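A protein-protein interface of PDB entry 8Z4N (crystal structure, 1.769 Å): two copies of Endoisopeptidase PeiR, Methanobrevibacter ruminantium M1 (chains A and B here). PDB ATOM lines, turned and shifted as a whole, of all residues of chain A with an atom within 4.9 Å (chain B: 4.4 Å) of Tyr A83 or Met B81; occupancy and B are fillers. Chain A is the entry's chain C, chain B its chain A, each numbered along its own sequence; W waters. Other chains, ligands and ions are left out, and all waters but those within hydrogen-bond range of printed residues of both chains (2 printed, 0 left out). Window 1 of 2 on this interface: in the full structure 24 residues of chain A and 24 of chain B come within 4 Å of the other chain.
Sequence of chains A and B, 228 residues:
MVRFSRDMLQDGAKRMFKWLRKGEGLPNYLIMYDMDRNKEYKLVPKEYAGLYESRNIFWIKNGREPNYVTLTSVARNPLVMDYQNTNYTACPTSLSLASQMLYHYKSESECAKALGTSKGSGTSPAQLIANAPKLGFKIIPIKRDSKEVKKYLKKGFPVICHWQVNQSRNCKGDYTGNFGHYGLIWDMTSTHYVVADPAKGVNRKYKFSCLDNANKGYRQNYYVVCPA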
ATOM      1  N   MET A  81      15.769 -10.362 -12.171  1.00  0.00           N
ATOM      2  CA  MET A  81      16.070 -10.515 -10.746  1.00  0.00           C
ATOM      3  C   MET A  81      14.892 -10.135  -9.876  1.00  0.00           C
ATOM      4  O   MET A  81      14.228  -9.130 -10.084  1.00  0.00           O
ATOM      5  CB  MET A  81      17.297  -9.694 -10.334  1.00  0.00           C
ATOM      6  CG  MET A  81      17.979 -10.151  -8.997  1.00  0.00           C
ATOM      7  SD  MET A  81      17.856 -11.910  -8.566  1.00  0.00           S
ATOM      8  CE  MET A  81      18.310 -11.904  -6.837  1.00  0.00           C
ATOM      9  N   ASP A  82      14.630 -10.968  -8.885  1.00  0.00           N
ATOM     10  CA  ASP A  82      13.529 -10.757  -7.967  1.00  0.00           C
ATOM     11  C   ASP A  82      14.030 -11.154  -6.586  1.00  0.00           C
ATOM     12  O   ASP A  82      14.493 -12.270  -6.389  1.00  0.00           O
ATOM     13  CB  ASP A  82      12.307 -11.577  -8.391  1.00  0.00           C
ATOM     14  CG  ASP A  82      11.075 -11.242  -7.592  1.00  0.00           C
ATOM     15  OD1 ASP A  82      11.010 -10.150  -6.980  1.00  0.00           O
ATOM     16  OD2 ASP A  82      10.166 -12.085  -7.576  1.00  0.00           O
ATOM     17  N   TYR A  83      14.038 -10.213  -5.672  1.00  0.00           N
ATOM     18  CA  TYR A  83      14.582 -10.452  -4.347  1.00  0.00           C
ATOM     19  C   TYR A  83      13.470 -10.928  -3.422  1.00  0.00           C
ATOM     20  O   TYR A  83      12.309 -10.604  -3.639  1.00  0.00           O
ATOM     21  CB  TYR A  83      15.252  -9.159  -3.845  1.00  0.00           C
ATOM     22  CG  TYR A  83      16.313  -8.552  -4.763  1.00  0.00           C
ATOM     23  CD1 TYR A  83      17.630  -8.939  -4.658  1.00  0.00           C
ATOM     24  CD2 TYR A  83      16.011  -7.546  -5.689  1.00  0.00           C
ATOM     25  CE1 TYR A  83      18.629  -8.386  -5.463  1.00  0.00           C
ATOM     26  CE2 TYR A  83      17.013  -6.977  -6.518  1.00  0.00           C
ATOM     27  CZ  TYR A  83      18.327  -7.407  -6.387  1.00  0.00           C
ATOM     28  OH  TYR A  83      19.387  -6.890  -7.143  1.00  0.00           O
ATOM     29  N   GLN A  84      13.859 -11.658  -2.384  1.00  0.00           N
ATOM     30  CA  GLN A  84      12.895 -12.134  -1.376  1.00  0.00           C
ATOM     31  C   GLN A  84      12.413 -10.916  -0.602  1.00  0.00           C
ATOM     32  O   GLN A  84      13.216 -10.044  -0.349  1.00  0.00           O
ATOM     33  CB  GLN A  84      13.519 -13.202  -0.487  1.00  0.00           C
ATOM     34  CG  GLN A  84      14.661 -12.724   0.387  1.00  0.00           C
ATOM     35  CD  GLN A  84      15.368 -13.897   1.013  1.00  0.00           C
ATOM     36  OE1 GLN A  84      16.222 -14.514   0.416  1.00  0.00           O
ATOM     37  NE2 GLN A  84      14.978 -14.245   2.215  1.00  0.00           N
ATOM     38  N   ASN A  85      11.118 -10.884  -0.316  1.00  0.00           N
ATOM     39  CA  ASN A  85      10.499  -9.714   0.348  1.00  0.00           C
ATOM     40  C   ASN A  85      10.522  -9.860   1.875  1.00  0.00           C
ATOM     41  O   ASN A  85      10.075  -8.952   2.527  1.00  0.00           O
ATOM     42  CB  ASN A  85       9.107  -9.425  -0.222  1.00  0.00           C
ATOM     43  CG  ASN A  85       9.019  -9.260  -1.732  1.00  0.00           C
ATOM     44  OD1 ASN A  85       9.860  -8.639  -2.382  1.00  0.00           O
ATOM     45  ND2 ASN A  85       7.945  -9.770  -2.303  1.00  0.00           N
ATOM     46  N   THR A  93      10.723 -17.523  -3.428  1.00  0.00           N
ATOM     47  CA  THR A  93      11.329 -16.622  -4.400  1.00  0.00           C
ATOM     48  C   THR A  93      12.124 -17.397  -5.441  1.00  0.00           C
ATOM     49  O   THR A  93      12.087 -17.061  -6.638  1.00  0.00           O
ATOM     50  CB  THR A  93      12.237 -15.586  -3.721  1.00  0.00           C
ATOM     51  OG1 THR A  93      11.588 -14.965  -2.600  1.00  0.00           O
ATOM     52  CG2 THR A  93      12.647 -14.481  -4.734  1.00  0.00           C
ATOM     53  N   GLU A 108       6.202 -14.417  -6.082  1.00  0.00           N
ATOM     54  CA  GLU A 108       6.752 -14.919  -4.830  1.00  0.00           C
ATOM     55  C   GLU A 108       5.636 -15.181  -3.819  1.00  0.00           C
ATOM     56  O   GLU A 108       5.638 -16.201  -3.125  1.00  0.00           O
ATOM     57  CB  GLU A 108       7.752 -13.914  -4.265  1.00  0.00           C
ATOM     58  CG  GLU A 108       8.014 -14.151  -2.795  1.00  0.00           C
ATOM     59  CD  GLU A 108       9.054 -13.225  -2.195  1.00  0.00           C
ATOM     60  OE1 GLU A 108       9.793 -12.577  -2.958  1.00  0.00           O
ATOM     61  OE2 GLU A 108       9.120 -13.142  -0.948  1.00  0.00           O
ATOM     62  N   PRO A 198      18.165 -14.948  -3.880  1.00  0.00           N
ATOM     63  CA  PRO A 198      17.141 -13.928  -3.604  1.00  0.00           C
ATOM     64  C   PRO A 198      17.559 -12.907  -2.553  1.00  0.00           C
ATOM     65  O   PRO A 198      16.855 -11.901  -2.382  1.00  0.00           O
ATOM     66  CB  PRO A 198      15.963 -14.759  -3.079  1.00  0.00           C
ATOM     67  CG  PRO A 198      16.227 -16.130  -3.556  1.00  0.00           C
ATOM     68  CD  PRO A 198      17.714 -16.284  -3.471  1.00  0.00           C
ATOM     69  N   LYS A 200      20.897 -11.634  -2.524  1.00  0.00           N
ATOM     70  CA  LYS A 200      22.185 -11.054  -2.909  1.00  0.00           C
ATOM     71  C   LYS A 200      22.221 -10.545  -4.347  1.00  0.00           C
ATOM     72  O   LYS A 200      22.605  -9.395  -4.587  1.00  0.00           O
ATOM     73  CB  LYS A 200      23.312 -12.083  -2.697  1.00  0.00           C
ATOM     74  CG  LYS A 200      23.626 -12.395  -1.230  1.00  0.00           C
ATOM     75  CD  LYS A 200      24.505 -11.359  -0.578  1.00  0.00           C
ATOM     76  CE  LYS A 200      25.612 -10.923  -1.482  1.00  0.00           C
ATOM     77  NZ  LYS A 200      26.158  -9.632  -0.972  1.00  0.00           N
ATOM     78  N   GLY A 201      21.814 -11.357  -5.310  1.00  0.00           N
ATOM     79  CA  GLY A 201      21.945 -10.935  -6.695  1.00  0.00           C
ATOM     80  C   GLY A 201      21.714 -12.099  -7.623  1.00  0.00           C
ATOM     81  O   GLY A 201      21.651 -13.260  -7.202  1.00  0.00           O
ATOM     82  N   ILE B  57      17.395  -4.079  -0.271  1.00  0.00           N
ATOM     83  CA  ILE B  57      16.541  -5.147  -0.802  1.00  0.00           C
ATOM     84  C   ILE B  57      15.150  -5.058  -0.186  1.00  0.00           C
ATOM     85  O   ILE B  57      14.136  -5.043  -0.896  1.00  0.00           O
ATOM     86  CB  ILE B  57      17.181  -6.522  -0.533  1.00  0.00           C
ATOM     87  CG1 ILE B  57      18.474  -6.660  -1.335  1.00  0.00           C
ATOM     88  CG2 ILE B  57      16.200  -7.653  -0.844  1.00  0.00           C
ATOM     89  CD1 ILE B  57      19.224  -7.952  -1.070  1.00  0.00           C
ATOM     90  N   LYS B  61      11.826  -3.913  -2.411  1.00  0.00           N
ATOM     91  CA  LYS B  61      10.759  -4.904  -2.656  1.00  0.00           C
ATOM     92  C   LYS B  61       9.454  -4.568  -1.931  1.00  0.00           C
ATOM     93  O   LYS B  61       8.418  -4.864  -2.477  1.00  0.00           O
ATOM     94  CB  LYS B  61      11.304  -6.276  -2.278  1.00  0.00           C
ATOM     95  CG  LYS B  61      12.437  -6.717  -3.185  1.00  0.00           C
ATOM     96  CD  LYS B  61      12.153  -6.472  -4.657  1.00  0.00           C
ATOM     97  CE  LYS B  61      11.447  -7.620  -5.342  1.00  0.00           C
ATOM     98  NZ  LYS B  61      11.418  -7.492  -6.815  1.00  0.00           N
ATOM     99  N   LEU B  79      24.416  -1.494  -3.665  1.00  0.00           N
ATOM    100  CA  LEU B  79      23.503  -1.380  -4.795  1.00  0.00           C
ATOM    101  C   LEU B  79      22.638  -2.629  -4.925  1.00  0.00           C
ATOM    102  O   LEU B  79      23.146  -3.751  -4.873  1.00  0.00           O
ATOM    103  CB  LEU B  79      24.288  -1.189  -6.086  1.00  0.00           C
ATOM    104  CG  LEU B  79      23.476  -1.069  -7.379  1.00  0.00           C
ATOM    105  CD1 LEU B  79      22.566   0.144  -7.338  1.00  0.00           C
ATOM    106  CD2 LEU B  79      24.441  -0.963  -8.534  1.00  0.00           C
ATOM    107  N   VAL B  80      21.341  -2.414  -5.121  1.00  0.00           N
ATOM    108  CA  VAL B  80      20.353  -3.464  -5.368  1.00  0.00           C
ATOM    109  C   VAL B  80      19.671  -3.129  -6.690  1.00  0.00           C
ATOM    110  O   VAL B  80      19.179  -2.005  -6.868  1.00  0.00           O
ATOM    111  CB  VAL B  80      19.336  -3.539  -4.209  1.00  0.00           C
ATOM    112  CG1 VAL B  80      18.196  -4.529  -4.511  1.00  0.00           C
ATOM    113  CG2 VAL B  80      20.043  -3.874  -2.869  1.00  0.00           C
ATOM    114  N   MET B  81      19.665  -4.071  -7.634  1.00  0.00           N
ATOM    115  CA  MET B  81      19.043  -3.758  -8.924  1.00  0.00           C
ATOM    116  C   MET B  81      17.606  -3.319  -8.704  1.00  0.00           C
ATOM    117  O   MET B  81      16.857  -3.955  -7.956  1.00  0.00           O
ATOM    118  CB  MET B  81      19.074  -4.958  -9.881  1.00  0.00           C
ATOM    119  CG  MET B  81      18.557  -4.630 -11.317  1.00  0.00           C
ATOM    120  SD  MET B  81      19.313  -3.094 -11.999  1.00  0.00           S
ATOM    121  CE  MET B  81      17.959  -2.443 -12.958  1.00  0.00           C
ATOM    122  N   ASP B  82      17.220  -2.234  -9.362  1.00  0.00           N
ATOM    123  CA  ASP B  82      15.866  -1.710  -9.269  1.00  0.00           C
ATOM    124  C   ASP B  82      15.437  -1.356 -10.691  1.00  0.00           C
ATOM    125  O   ASP B  82      16.075  -0.539 -11.362  1.00  0.00           O
ATOM    126  CB  ASP B  82      15.834  -0.500  -8.345  1.00  0.00           C
ATOM    127  CG  ASP B  82      14.452   0.035  -8.133  1.00  0.00           C
ATOM    128  OD1 ASP B  82      13.464  -0.723  -8.241  1.00  0.00           O
ATOM    129  OD2 ASP B  82      14.375   1.237  -7.818  1.00  0.00           O
ATOM    130  N   TYR B  83      14.389  -1.997 -11.165  1.00  0.00           N
ATOM    131  CA  TYR B  83      13.968  -1.841 -12.551  1.00  0.00           C
ATOM    132  C   TYR B  83      12.974  -0.698 -12.654  1.00  0.00           C
ATOM    133  O   TYR B  83      12.317  -0.347 -11.674  1.00  0.00           O
ATOM    134  CB  TYR B  83      13.353  -3.153 -13.072  1.00  0.00           C
ATOM    135  CG  TYR B  83      14.287  -4.370 -13.127  1.00  0.00           C
ATOM    136  CD1 TYR B  83      15.058  -4.598 -14.239  1.00  0.00           C
ATOM    137  CD2 TYR B  83      14.344  -5.326 -12.084  1.00  0.00           C
ATOM    138  CE1 TYR B  83      15.902  -5.726 -14.337  1.00  0.00           C
ATOM    139  CE2 TYR B  83      15.206  -6.455 -12.159  1.00  0.00           C
ATOM    140  CZ  TYR B  83      15.981  -6.654 -13.309  1.00  0.00           C
ATOM    141  OH  TYR B  83      16.844  -7.769 -13.486  1.00  0.00           O
ATOM    142  N   ASP B 197      21.234  -0.769 -15.996  1.00  0.00           N
ATOM    143  CA  ASP B 197      20.220  -0.343 -16.943  1.00  0.00           C
ATOM    144  C   ASP B 197      18.840  -0.683 -16.399  1.00  0.00           C
ATOM    145  O   ASP B 197      18.484  -1.870 -16.353  1.00  0.00           O
ATOM    146  CB  ASP B 197      20.453  -1.029 -18.311  1.00  0.00           C
ATOM    147  CG  ASP B 197      19.441  -0.618 -19.375  1.00  0.00           C
ATOM    148  OD1 ASP B 197      18.340  -0.190 -18.982  1.00  0.00           O
ATOM    149  OD2 ASP B 197      19.719  -0.748 -20.621  1.00  0.00           O
ATOM    150  N   PRO B 198      17.991   0.311 -16.117  1.00  0.00           N
ATOM    151  CA  PRO B 198      16.705   0.026 -15.451  1.00  0.00           C
ATOM    152  C   PRO B 198      15.758  -0.817 -16.287  1.00  0.00           C
ATOM    153  O   PRO B 198      14.712  -1.230 -15.767  1.00  0.00           O
ATOM    154  CB  PRO B 198      16.104   1.422 -15.224  1.00  0.00           C
ATOM    155  CG  PRO B 198      17.270   2.386 -15.380  1.00  0.00           C
ATOM    156  CD  PRO B 198      18.170   1.755 -16.390  1.00  0.00           C
ATOM    157  N   GLY B 201      19.213  -4.823 -16.693  1.00  0.00           N
ATOM    158  CA  GLY B 201      19.970  -5.544 -15.690  1.00  0.00           C
ATOM    159  C   GLY B 201      21.024  -4.655 -15.086  1.00  0.00           C
ATOM    160  O   GLY B 201      21.341  -3.570 -15.605  1.00  0.00           O
ATOM    161  N   VAL B 202      21.599  -5.148 -13.981  1.00  0.00           N
ATOM    162  CA  VAL B 202      22.494  -4.311 -13.176  1.00  0.00           C
ATOM    163  C   VAL B 202      23.888  -4.214 -13.766  1.00  0.00           C
ATOM    164  O   VAL B 202      24.665  -3.341 -13.368  1.00  0.00           O
ATOM    165  CB  VAL B 202      22.576  -4.878 -11.744  1.00  0.00           C
ATOM    166  CG1 VAL B 202      23.488  -6.098 -11.714  1.00  0.00           C
ATOM    167  CG2 VAL B 202      23.039  -3.815 -10.743  1.00  0.00           C
HETATM  168  O   HOH W   1      13.678  -7.390  -8.028  1.00  0.00           O
HETATM  169  O   HOH W   2      22.492  -6.578  -4.876  1.00  0.00           O
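Hydrophobic or aromatic side chains of chain A within 4 Å of the printed part of chain B: Met A81 and Tyr A83. Among the printed residues, Asp or Glu carboxylates within 4 Å of a Lys or Arg side-chain nitrogen of the other chain: Asp A82 with Lys B61.
Water W1 lies within hydrogen-bond range of NZ of Lys B61 and O of Met A81. Water W2 bridges O of Lys A200 (2.8 Å) and O of Leu B79 (2.9 Å).
Among the printed residues, merely in contact across the chains: Asn A85 with Lys B61 (2.8 Å), Tyr A83 with Val B80 (3.4 Å), Tyr A83 with Ile B57 (3.5 Å), Tyr A83 with Lys B61 (3.5 Å) and Gln A84 with Ile B57 (3.9 Å).
Met A81 touches Tyr B83, and with the chains exchanged Tyr A83 touches Met B81. 5 positions are printed for both chains.
Of the printed residues of chain A, Met B81 touches Tyr A83 (2.9 Å). Of the printed residues of chain A, Tyr B83 touches Met A81. Printed residues of chain B within 4 Å of Met A81: Tyr B83 (3.1 Å). Printed residues of chain A within 4 Å of Ile B57: Tyr A83 and Gln A84. Of the printed residues of chain B, Gln A84 touches Ile B57 (3.9 Å). Of the printed residues of chain B, Asp A82 touches Lys B61. The nearest printed residue of chain A that does not touch Tyr B83 is Asp A82 (5.6 Å).
The side-chain sulfur (SD) of Met B81 sits close to the backbone NH (N) of Val B202, 3.7 Å away. OD1 of Asn A85 sits close to O of Tyr A83, at 3.4 Å. The backbone NH of Gln A84 is in hydrogen-bond range of the backbone carbonyl oxygen of Pro A198. The side-chain carboxylate (OE2) of Glu A108 lies within hydrogen-bond range of the backbone NH (N) of Asn A85, at 3.1 Å.
The side-chain amino group (NZ) of Lys B61 is in salt-bridge range of the side-chain carboxylate (OD1) of Asp A82 (2.7 Å). The backbone NH (N) of Met B81 sits at hydrogen-bond distance from the side-chain hydroxyl (OH) of Tyr A83, at 2.9 Å. The backbone NH (N) of Met A81 sits at hydrogen-bond distance from the side-chain hydroxyl (OH) of Tyr B83, at 3.1 Å.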
